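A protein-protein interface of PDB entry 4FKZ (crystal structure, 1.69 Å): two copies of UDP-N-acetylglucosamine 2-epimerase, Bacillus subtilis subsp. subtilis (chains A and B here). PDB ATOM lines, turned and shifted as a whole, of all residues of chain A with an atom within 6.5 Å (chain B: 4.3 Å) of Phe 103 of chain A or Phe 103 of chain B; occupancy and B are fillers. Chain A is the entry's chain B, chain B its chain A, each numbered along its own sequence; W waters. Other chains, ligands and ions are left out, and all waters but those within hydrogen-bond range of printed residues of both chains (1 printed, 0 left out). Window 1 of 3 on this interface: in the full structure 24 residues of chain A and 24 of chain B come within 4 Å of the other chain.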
ATOM      1  N   THR A  74     -30.010 -11.669  35.666  1.00  0.00           N
ATOM      2  CA  THR A  74     -29.535 -11.598  34.274  1.00  0.00           C
ATOM      3  C   THR A  74     -28.805 -10.291  34.014  1.00  0.00           C
ATOM      4  O   THR A  74     -27.701 -10.286  33.487  1.00  0.00           O
ATOM      5  CB  THR A  74     -30.696 -11.746  33.272  1.00  0.00           C
ATOM      6  OG1 THR A  74     -31.463 -12.913  33.585  1.00  0.00           O
ATOM      7  CG2 THR A  74     -30.150 -11.853  31.819  1.00  0.00           C
ATOM      8  N   VAL A  95     -18.760 -22.509  30.998  1.00  0.00           N
ATOM      9  CA  VAL A  95     -19.934 -22.358  31.866  1.00  0.00           C
ATOM     10  C   VAL A  95     -20.512 -23.718  32.186  1.00  0.00           C
ATOM     11  O   VAL A  95     -20.187 -24.723  31.527  1.00  0.00           O
ATOM     12  CB  VAL A  95     -21.032 -21.482  31.226  1.00  0.00           C
ATOM     13  CG1 VAL A  95     -20.552 -20.042  31.124  1.00  0.00           C
ATOM     14  CG2 VAL A  95     -21.442 -22.049  29.865  1.00  0.00           C
ATOM     15  N   HIS A  96     -21.378 -23.751  33.201  1.00  0.00           N
ATOM     16  CA  HIS A  96     -21.936 -24.993  33.687  1.00  0.00           C
ATOM     17  C   HIS A  96     -23.434 -25.059  33.710  1.00  0.00           C
ATOM     18  O   HIS A  96     -24.090 -24.250  34.372  1.00  0.00           O
ATOM     19  CB  HIS A  96     -21.470 -25.318  35.117  1.00  0.00           C
ATOM     20  CG  HIS A  96     -21.947 -26.663  35.561  1.00  0.00           C
ATOM     21  ND1 HIS A  96     -23.172 -26.858  36.105  1.00  0.00           N
ATOM     22  CD2 HIS A  96     -21.384 -27.931  35.385  1.00  0.00           C
ATOM     23  CE1 HIS A  96     -23.359 -28.172  36.311  1.00  0.00           C
ATOM     24  NE2 HIS A  96     -22.264 -28.829  35.851  1.00  0.00           N
ATOM     25  N   GLY A  97     -23.984 -26.062  33.040  1.00  0.00           N
ATOM     26  CA  GLY A  97     -25.359 -26.493  33.329  1.00  0.00           C
ATOM     27  C   GLY A  97     -26.434 -25.501  32.916  1.00  0.00           C
ATOM     28  O   GLY A  97     -26.560 -25.174  31.741  1.00  0.00           O
ATOM     29  N   ASP A  98     -27.221 -25.008  33.880  1.00  0.00           N
ATOM     30  CA  ASP A  98     -28.465 -24.345  33.487  1.00  0.00           C
ATOM     31  C   ASP A  98     -28.975 -23.215  34.383  1.00  0.00           C
ATOM     32  O   ASP A  98     -30.178 -22.945  34.392  1.00  0.00           O
ATOM     33  CB  ASP A  98     -29.569 -25.393  33.300  1.00  0.00           C
ATOM     34  CG  ASP A  98     -29.768 -26.274  34.519  1.00  0.00           C
ATOM     35  OD1 ASP A  98     -29.421 -25.859  35.655  1.00  0.00           O
ATOM     36  OD2 ASP A  98     -30.283 -27.400  34.344  1.00  0.00           O
ATOM     37  N   THR A  99     -28.071 -22.560  35.096  1.00  0.00           N
ATOM     38  CA  THR A  99     -28.470 -21.407  35.925  1.00  0.00           C
ATOM     39  C   THR A  99     -28.573 -20.135  35.084  1.00  0.00           C
ATOM     40  O   THR A  99     -28.162 -20.099  33.927  1.00  0.00           O
ATOM     41  CB  THR A  99     -27.508 -21.162  37.109  1.00  0.00           C
ATOM     42  OG1 THR A  99     -26.307 -20.560  36.629  1.00  0.00           O
ATOM     43  CG2 THR A  99     -27.181 -22.476  37.835  1.00  0.00           C
ATOM     44  N   THR A 100     -29.113 -19.073  35.673  1.00  0.00           N
ATOM     45  CA  THR A 100     -29.114 -17.788  34.998  1.00  0.00           C
ATOM     46  C   THR A 100     -27.692 -17.259  34.822  1.00  0.00           C
ATOM     47  O   THR A 100     -27.399 -16.588  33.824  1.00  0.00           O
ATOM     48  CB  THR A 100     -30.092 -16.802  35.679  1.00  0.00           C
ATOM     49  OG1 THR A 100     -31.398 -17.368  35.595  1.00  0.00           O
ATOM     50  CG2 THR A 100     -30.091 -15.452  34.996  1.00  0.00           C
ATOM     51  N   THR A 101     -26.793 -17.625  35.749  1.00  0.00           N
ATOM     52  CA  THR A 101     -25.361 -17.325  35.596  1.00  0.00           C
ATOM     53  C   THR A 101     -24.784 -18.018  34.355  1.00  0.00           C
ATOM     54  O   THR A 101     -24.026 -17.405  33.594  1.00  0.00           O
ATOM     55  CB  THR A 101     -24.548 -17.705  36.859  1.00  0.00           C
ATOM     56  OG1 THR A 101     -24.810 -16.743  37.892  1.00  0.00           O
ATOM     57  CG2 THR A 101     -23.043 -17.695  36.578  1.00  0.00           C
ATOM     58  N   THR A 102     -25.168 -19.273  34.143  1.00  0.00           N
ATOM     59  CA  THR A 102     -24.714 -20.038  32.960  1.00  0.00           C
ATOM     60  C   THR A 102     -25.039 -19.259  31.692  1.00  0.00           C
ATOM     61  O   THR A 102     -24.177 -19.046  30.815  1.00  0.00           O
ATOM     62  CB  THR A 102     -25.428 -21.413  32.874  1.00  0.00           C
ATOM     63  OG1 THR A 102     -25.378 -22.069  34.154  1.00  0.00           O
ATOM     64  CG2 THR A 102     -24.761 -22.313  31.793  1.00  0.00           C
ATOM     65  N   PHE A 103     -26.291 -18.838  31.591  1.00  0.00           N
ATOM     66  CA  PHE A 103     -26.734 -18.136  30.392  1.00  0.00           C
ATOM     67  C   PHE A 103     -26.124 -16.737  30.266  1.00  0.00           C
ATOM     68  O   PHE A 103     -25.585 -16.378  29.219  1.00  0.00           O
ATOM     69  CB  PHE A 103     -28.250 -18.063  30.294  1.00  0.00           C
ATOM     70  CG  PHE A 103     -28.703 -17.291  29.086  1.00  0.00           C
ATOM     71  CD1 PHE A 103     -28.289 -17.693  27.824  1.00  0.00           C
ATOM     72  CD2 PHE A 103     -29.475 -16.159  29.209  1.00  0.00           C
ATOM     73  CE1 PHE A 103     -28.647 -16.985  26.695  1.00  0.00           C
ATOM     74  CE2 PHE A 103     -29.855 -15.444  28.076  1.00  0.00           C
ATOM     75  CZ  PHE A 103     -29.441 -15.860  26.823  1.00  0.00           C
ATOM     76  N   ALA A 104     -26.209 -15.940  31.335  1.00  0.00           N
ATOM     77  CA  ALA A 104     -25.597 -14.610  31.319  1.00  0.00           C
ATOM     78  C   ALA A 104     -24.100 -14.641  31.015  1.00  0.00           C
ATOM     79  O   ALA A 104     -23.592 -13.767  30.320  1.00  0.00           O
ATOM     80  CB  ALA A 104     -25.867 -13.879  32.639  1.00  0.00           C
ATOM     81  N   GLY A 105     -23.392 -15.629  31.570  1.00  0.00           N
ATOM     82  CA  GLY A 105     -21.948 -15.806  31.325  1.00  0.00           C
ATOM     83  C   GLY A 105     -21.675 -16.077  29.850  1.00  0.00           C
ATOM     84  O   GLY A 105     -20.777 -15.469  29.249  1.00  0.00           O
ATOM     85  N   SER A 106     -22.468 -16.980  29.276  1.00  0.00           N
ATOM     86  CA  SER A 106     -22.352 -17.337  27.858  1.00  0.00           C
ATOM     87  C   SER A 106     -22.625 -16.124  26.980  1.00  0.00           C
ATOM     88  O   SER A 106     -21.893 -15.871  26.023  1.00  0.00           O
ATOM     89  CB  SER A 106     -23.320 -18.477  27.501  1.00  0.00           C
ATOM     90  OG  SER A 106     -23.066 -19.614  28.314  1.00  0.00           O
ATOM     91  N   LEU A 107     -23.661 -15.362  27.330  1.00  0.00           N
ATOM     92  CA  LEU A 107     -24.064 -14.189  26.561  1.00  0.00           C
ATOM     93  C   LEU A 107     -23.008 -13.089  26.632  1.00  0.00           C
ATOM     94  O   LEU A 107     -22.654 -12.484  25.604  1.00  0.00           O
ATOM     95  CB  LEU A 107     -25.433 -13.689  27.035  1.00  0.00           C
ATOM     96  CG  LEU A 107     -26.063 -12.567  26.198  1.00  0.00           C
ATOM     97  CD1 LEU A 107     -26.555 -13.130  24.877  1.00  0.00           C
ATOM     98  CD2 LEU A 107     -27.211 -11.941  26.988  1.00  0.00           C
ATOM     99  N   ALA A 108     -22.480 -12.836  27.836  1.00  0.00           N
ATOM    100  CA  ALA A 108     -21.412 -11.850  27.986  1.00  0.00           C
ATOM    101  C   ALA A 108     -20.164 -12.219  27.175  1.00  0.00           C
ATOM    102  O   ALA A 108     -19.570 -11.348  26.523  1.00  0.00           O
ATOM    103  CB  ALA A 108     -21.045 -11.657  29.461  1.00  0.00           C
ATOM    104  N   TYR A 111     -20.845 -11.626  23.497  1.00  0.00           N
ATOM    105  CA  TYR A 111     -20.814 -10.205  23.153  1.00  0.00           C
ATOM    106  C   TYR A 111     -19.384  -9.680  22.967  1.00  0.00           C
ATOM    107  O   TYR A 111     -19.176  -8.672  22.301  1.00  0.00           O
ATOM    108  CB  TYR A 111     -21.542  -9.371  24.207  1.00  0.00           C
ATOM    109  CG  TYR A 111     -23.061  -9.458  24.177  1.00  0.00           C
ATOM    110  CD1 TYR A 111     -23.741 -10.077  23.116  1.00  0.00           C
ATOM    111  CD2 TYR A 111     -23.830  -8.883  25.213  1.00  0.00           C
ATOM    112  CE1 TYR A 111     -25.129 -10.131  23.088  1.00  0.00           C
ATOM    113  CE2 TYR A 111     -25.219  -8.928  25.192  1.00  0.00           C
ATOM    114  CZ  TYR A 111     -25.861  -9.553  24.132  1.00  0.00           C
ATOM    115  OH  TYR A 111     -27.232  -9.604  24.112  1.00  0.00           O
ATOM    116  N   LEU A 136     -34.902 -23.352  29.445  1.00  0.00           N
ATOM    117  CA  LEU A 136     -34.460 -22.387  28.447  1.00  0.00           C
ATOM    118  C   LEU A 136     -33.031 -21.892  28.663  1.00  0.00           C
ATOM    119  O   LEU A 136     -32.335 -21.615  27.699  1.00  0.00           O
ATOM    120  CB  LEU A 136     -35.473 -21.237  28.258  1.00  0.00           C
ATOM    121  CG  LEU A 136     -36.838 -21.618  27.637  1.00  0.00           C
ATOM    122  CD1 LEU A 136     -37.367 -20.402  26.912  1.00  0.00           C
ATOM    123  CD2 LEU A 136     -36.815 -22.800  26.671  1.00  0.00           C
ATOM    124  N   ASN A 137     -32.569 -21.794  29.915  1.00  0.00           N
ATOM    125  CA  ASN A 137     -31.177 -21.424  30.150  1.00  0.00           C
ATOM    126  C   ASN A 137     -30.237 -22.371  29.416  1.00  0.00           C
ATOM    127  O   ASN A 137     -29.311 -21.920  28.739  1.00  0.00           O
ATOM    128  CB  ASN A 137     -30.831 -21.438  31.645  1.00  0.00           C
ATOM    129  CG  ASN A 137     -31.386 -20.240  32.387  1.00  0.00           C
ATOM    130  OD1 ASN A 137     -31.781 -19.248  31.775  1.00  0.00           O
ATOM    131  ND2 ASN A 137     -31.411 -20.324  33.717  1.00  0.00           N
ATOM    132  N   ARG A 138     -30.475 -23.674  29.545  1.00  0.00           N
ATOM    133  CA  ARG A 138     -29.586 -24.631  28.887  1.00  0.00           C
ATOM    134  C   ARG A 138     -29.760 -24.640  27.363  1.00  0.00           C
ATOM    135  O   ARG A 138     -28.789 -24.834  26.647  1.00  0.00           O
ATOM    136  CB  ARG A 138     -29.655 -26.038  29.490  1.00  0.00           C
ATOM    137  CG  ARG A 138     -31.018 -26.714  29.502  1.00  0.00           C
ATOM    138  CD  ARG A 138     -31.129 -27.583  30.746  1.00  0.00           C
ATOM    139  NE  ARG A 138     -32.413 -28.281  30.811  1.00  0.00           N
ATOM    140  CZ  ARG A 138     -32.968 -28.761  31.921  1.00  0.00           C
ATOM    141  NH1 ARG A 138     -32.343 -28.648  33.092  1.00  0.00           N
ATOM    142  NH2 ARG A 138     -34.143 -29.381  31.853  1.00  0.00           N
ATOM    143  N   MET A 140     -30.711 -21.969  25.446  1.00  0.00           N
ATOM    144  CA  MET A 140     -30.086 -20.742  24.942  1.00  0.00           C
ATOM    145  C   MET A 140     -28.568 -20.787  25.080  1.00  0.00           C
ATOM    146  O   MET A 140     -27.844 -20.341  24.188  1.00  0.00           O
ATOM    147  CB  MET A 140     -30.680 -19.497  25.615  1.00  0.00           C
ATOM    148  CG  MET A 140     -32.160 -19.316  25.318  1.00  0.00           C
ATOM    149  SD  MET A 140     -32.817 -17.804  26.063  1.00  0.00           S
ATOM    150  CE  MET A 140     -32.595 -18.090  27.817  1.00  0.00           C
ATOM    151  N   THR A 141     -28.062 -21.377  26.166  1.00  0.00           N
ATOM    152  CA  THR A 141     -26.617 -21.584  26.277  1.00  0.00           C
ATOM    153  C   THR A 141     -26.114 -22.475  25.144  1.00  0.00           C
ATOM    154  O   THR A 141     -25.049 -22.213  24.570  1.00  0.00           O
ATOM    155  CB  THR A 141     -26.239 -22.170  27.651  1.00  0.00           C
ATOM    156  OG1 THR A 141     -26.571 -21.197  28.651  1.00  0.00           O
ATOM    157  CG2 THR A 141     -24.740 -22.467  27.743  1.00  0.00           C
ATOM    158  N   ILE A 144     -25.250 -20.668  21.966  1.00  0.00           N
ATOM    159  CA  ILE A 144     -24.028 -19.873  22.024  1.00  0.00           C
ATOM    160  C   ILE A 144     -22.776 -20.770  21.987  1.00  0.00           C
ATOM    161  O   ILE A 144     -21.791 -20.460  21.312  1.00  0.00           O
ATOM    162  CB  ILE A 144     -24.015 -19.000  23.307  1.00  0.00           C
ATOM    163  CG1 ILE A 144     -25.106 -17.917  23.222  1.00  0.00           C
ATOM    164  CG2 ILE A 144     -22.658 -18.328  23.505  1.00  0.00           C
ATOM    165  CD1 ILE A 144     -25.435 -17.248  24.558  1.00  0.00           C
ATOM    166  N   THR B  99     -33.121  -8.332  16.307  1.00  0.00           N
ATOM    167  CA  THR B  99     -32.403  -7.279  17.030  1.00  0.00           C
ATOM    168  C   THR B  99     -32.240  -7.688  18.494  1.00  0.00           C
ATOM    169  O   THR B  99     -32.873  -8.636  18.960  1.00  0.00           O
ATOM    170  CB  THR B  99     -33.102  -5.895  17.005  1.00  0.00           C
ATOM    171  OG1 THR B  99     -34.285  -5.940  17.809  1.00  0.00           O
ATOM    172  CG2 THR B  99     -33.480  -5.479  15.591  1.00  0.00           C
ATOM    173  N   THR B 100     -31.403  -6.945  19.206  1.00  0.00           N
ATOM    174  CA  THR B 100     -31.254  -7.153  20.640  1.00  0.00           C
ATOM    175  C   THR B 100     -32.572  -6.864  21.356  1.00  0.00           C
ATOM    176  O   THR B 100     -32.909  -7.533  22.321  1.00  0.00           O
ATOM    177  CB  THR B 100     -30.054  -6.366  21.191  1.00  0.00           C
ATOM    178  OG1 THR B 100     -28.866  -6.852  20.548  1.00  0.00           O
ATOM    179  CG2 THR B 100     -29.911  -6.589  22.689  1.00  0.00           C
ATOM    180  N   THR B 101     -33.347  -5.898  20.857  1.00  0.00           N
ATOM    181  CA  THR B 101     -34.704  -5.700  21.364  1.00  0.00           C
ATOM    182  C   THR B 101     -35.565  -6.957  21.198  1.00  0.00           C
ATOM    183  O   THR B 101     -36.302  -7.322  22.107  1.00  0.00           O
ATOM    184  CB  THR B 101     -35.386  -4.476  20.698  1.00  0.00           C
ATOM    185  OG1 THR B 101     -34.813  -3.270  21.221  1.00  0.00           O
ATOM    186  CG2 THR B 101     -36.877  -4.445  20.984  1.00  0.00           C
ATOM    187  N   THR B 102     -35.492  -7.605  20.028  1.00  0.00           N
ATOM    188  CA  THR B 102     -36.237  -8.840  19.797  1.00  0.00           C
ATOM    189  C   THR B 102     -35.958  -9.860  20.890  1.00  0.00           C
ATOM    190  O   THR B 102     -36.887 -10.425  21.485  1.00  0.00           O
ATOM    191  CB  THR B 102     -35.840  -9.477  18.448  1.00  0.00           C
ATOM    192  OG1 THR B 102     -35.847  -8.462  17.438  1.00  0.00           O
ATOM    193  CG2 THR B 102     -36.803 -10.601  18.081  1.00  0.00           C
ATOM    194  N   PHE B 103     -34.671 -10.091  21.126  1.00  0.00           N
ATOM    195  CA  PHE B 103     -34.253 -11.067  22.107  1.00  0.00           C
ATOM    196  C   PHE B 103     -34.623 -10.651  23.533  1.00  0.00           C
ATOM    197  O   PHE B 103     -35.235 -11.432  24.269  1.00  0.00           O
ATOM    198  CB  PHE B 103     -32.761 -11.361  21.995  1.00  0.00           C
ATOM    199  CG  PHE B 103     -32.271 -12.232  23.109  1.00  0.00           C
ATOM    200  CD1 PHE B 103     -32.792 -13.509  23.263  1.00  0.00           C
ATOM    201  CD2 PHE B 103     -31.370 -11.747  24.032  1.00  0.00           C
ATOM    202  CE1 PHE B 103     -32.380 -14.317  24.310  1.00  0.00           C
ATOM    203  CE2 PHE B 103     -30.956 -12.548  25.088  1.00  0.00           C
ATOM    204  CZ  PHE B 103     -31.471 -13.821  25.220  1.00  0.00           C
ATOM    205  N   ALA B 104     -34.270  -9.426  23.915  1.00  0.00           N
ATOM    206  CA  ALA B 104     -34.613  -8.942  25.262  1.00  0.00           C
ATOM    207  C   ALA B 104     -36.120  -8.947  25.527  1.00  0.00           C
ATOM    208  O   ALA B 104     -36.549  -9.296  26.631  1.00  0.00           O
ATOM    209  CB  ALA B 104     -34.024  -7.564  25.499  1.00  0.00           C
ATOM    210  N   GLY B 105     -36.917  -8.579  24.518  1.00  0.00           N
ATOM    211  CA  GLY B 105     -38.379  -8.634  24.616  1.00  0.00           C
ATOM    212  C   GLY B 105     -38.889 -10.039  24.876  1.00  0.00           C
ATOM    213  O   GLY B 105     -39.732 -10.252  25.749  1.00  0.00           O
ATOM    214  N   SER B 106     -38.360 -11.001  24.119  1.00  0.00           N
ATOM    215  CA  SER B 106     -38.719 -12.406  24.273  1.00  0.00           C
ATOM    216  C   SER B 106     -38.368 -12.914  25.663  1.00  0.00           C
ATOM    217  O   SER B 106     -39.136 -13.642  26.291  1.00  0.00           O
ATOM    218  CB  SER B 106     -37.937 -13.237  23.247  1.00  0.00           C
ATOM    219  OG  SER B 106     -38.385 -12.881  21.963  1.00  0.00           O
ATOM    220  N   LEU B 107     -37.189 -12.531  26.119  1.00  0.00           N
ATOM    221  CA  LEU B 107     -36.674 -12.997  27.404  1.00  0.00           C
ATOM    222  C   LEU B 107     -37.498 -12.406  28.546  1.00  0.00           C
ATOM    223  O   LEU B 107     -37.854 -13.112  29.497  1.00  0.00           O
ATOM    224  CB  LEU B 107     -35.197 -12.622  27.560  1.00  0.00           C
ATOM    225  CG  LEU B 107     -34.434 -13.227  28.754  1.00  0.00           C
ATOM    226  CD1 LEU B 107     -34.315 -14.751  28.652  1.00  0.00           C
ATOM    227  CD2 LEU B 107     -33.063 -12.563  28.880  1.00  0.00           C
ATOM    228  N   ASN B 137     -29.337 -13.734  18.080  1.00  0.00           N
ATOM    229  CA  ASN B 137     -30.600 -13.135  18.521  1.00  0.00           C
ATOM    230  C   ASN B 137     -31.812 -13.908  18.014  1.00  0.00           C
ATOM    231  O   ASN B 137     -32.714 -14.254  18.784  1.00  0.00           O
ATOM    232  CB  ASN B 137     -30.716 -11.673  18.079  1.00  0.00           C
ATOM    233  CG  ASN B 137     -29.848 -10.730  18.885  1.00  0.00           C
ATOM    234  OD1 ASN B 137     -29.371 -11.056  19.975  1.00  0.00           O
ATOM    235  ND2 ASN B 137     -29.665  -9.529  18.360  1.00  0.00           N
ATOM    236  N   MET B 140     -31.839 -17.606  19.648  1.00  0.00           N
ATOM    237  CA  MET B 140     -32.298 -17.605  21.039  1.00  0.00           C
ATOM    238  C   MET B 140     -33.770 -17.228  21.152  1.00  0.00           C
ATOM    239  O   MET B 140     -34.498 -17.823  21.947  1.00  0.00           O
ATOM    240  CB  MET B 140     -31.426 -16.699  21.912  1.00  0.00           C
ATOM    241  CG  MET B 140     -29.996 -17.200  22.039  1.00  0.00           C
ATOM    242  SD  MET B 140     -28.884 -16.145  22.994  1.00  0.00           S
ATOM    243  CE  MET B 140     -28.962 -14.564  22.140  1.00  0.00           C
ATOM    244  N   THR B 141     -34.207 -16.251  20.355  1.00  0.00           N
ATOM    245  CA  THR B 141     -35.630 -15.903  20.302  1.00  0.00           C
ATOM    246  C   THR B 141     -36.442 -17.129  19.917  1.00  0.00           C
ATOM    247  O   THR B 141     -37.507 -17.408  20.503  1.00  0.00           O
ATOM    248  CB  THR B 141     -35.882 -14.735  19.325  1.00  0.00           C
ATOM    249  OG1 THR B 141     -35.238 -13.563  19.846  1.00  0.00           O
ATOM    250  CG2 THR B 141     -37.375 -14.461  19.164  1.00  0.00           C
HETATM  251  O   HOH W   1     -27.997  -9.200  21.410  1.00  0.00           O
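Phe 103 of chain A touches its own counterpart, Phe 103 of chain B. Phe 103 of chain A touches Met 140 of chain B, and with the chains exchanged Met 140 of chain A touches Phe 103 of chain B. Leu 107 of chain A touches Met 140 of chain B, and with the chains exchanged Met 140 of chain A touches Leu 107 of chain B. Positions printed for both chains: 99, 100, 101, 102, 103, 104, 105, 106, 107, 137, 140 and 141. Of the 6 pairs that touch across the chains among the printed residues, 5 have their exchanged pair printed and touching as well.
Among the printed residues, pairs that only touch across the chains: Phe 103 of chain A with Phe 103 of chain B (3.3 Å), Phe 103 of chain A with Met 140 of chain B (3.8 Å), Met 140 of chain A with Leu 107 of chain B (3.8 Å), Leu 107 of chain A with Met 140 of chain B (3.9 Å), Met 140 of chain A with Phe 103 of chain B (3.9 Å) and Ile 144 of chain A with Met 140 of chain B (3.9 Å).
Water W1 lies within hydrogen-bond range of OG1 of Thr 100 of chain B (2.6 Å), OD1 of Asn 137 of chain B (2.7 Å) and OH of Tyr 111 of chain A (2.8 Å).
Of the 12 printed residues of chain B, 3 touch a printed residue of chain A. Along chain B the printed residues that touch a printed residue of chain A span positions 103 to 140. Hydrophobic or aromatic side chains of chain A that line the printed part of chain B: Phe 103, Leu 107, Met 140 and Ile 144. Among the printed residues, 6 pairs touch across the chains.
Of chain B, only Phe 103 and Met 140 come within 4 Å of Phe 103 of chain A. Of chain A, only Phe 103 (3.3 Å) and Met 140 (3.9 Å) come within 4 Å of Phe 103 of chain B. Of the printed residues of chain B, Ile 144 of chain A touches Met 140. Printed residues of chain B within 4 Å of Met 140 of chain A: Phe 103 and Leu 107. Printed residues of chain A within 4 Å of Leu 107 of chain B: Met 140. Of the printed residues of chain A, Met 140 of chain B touches Phe 103 (3.8 Å), Leu 107 (3.9 Å) and Ile 144 (3.9 Å). Ser 106 of chain B touches none of the printed residues of chain A. The nearest printed residue of chain B that does not touch Met 140 of chain A is Met 140 of chain B (4.3 Å).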
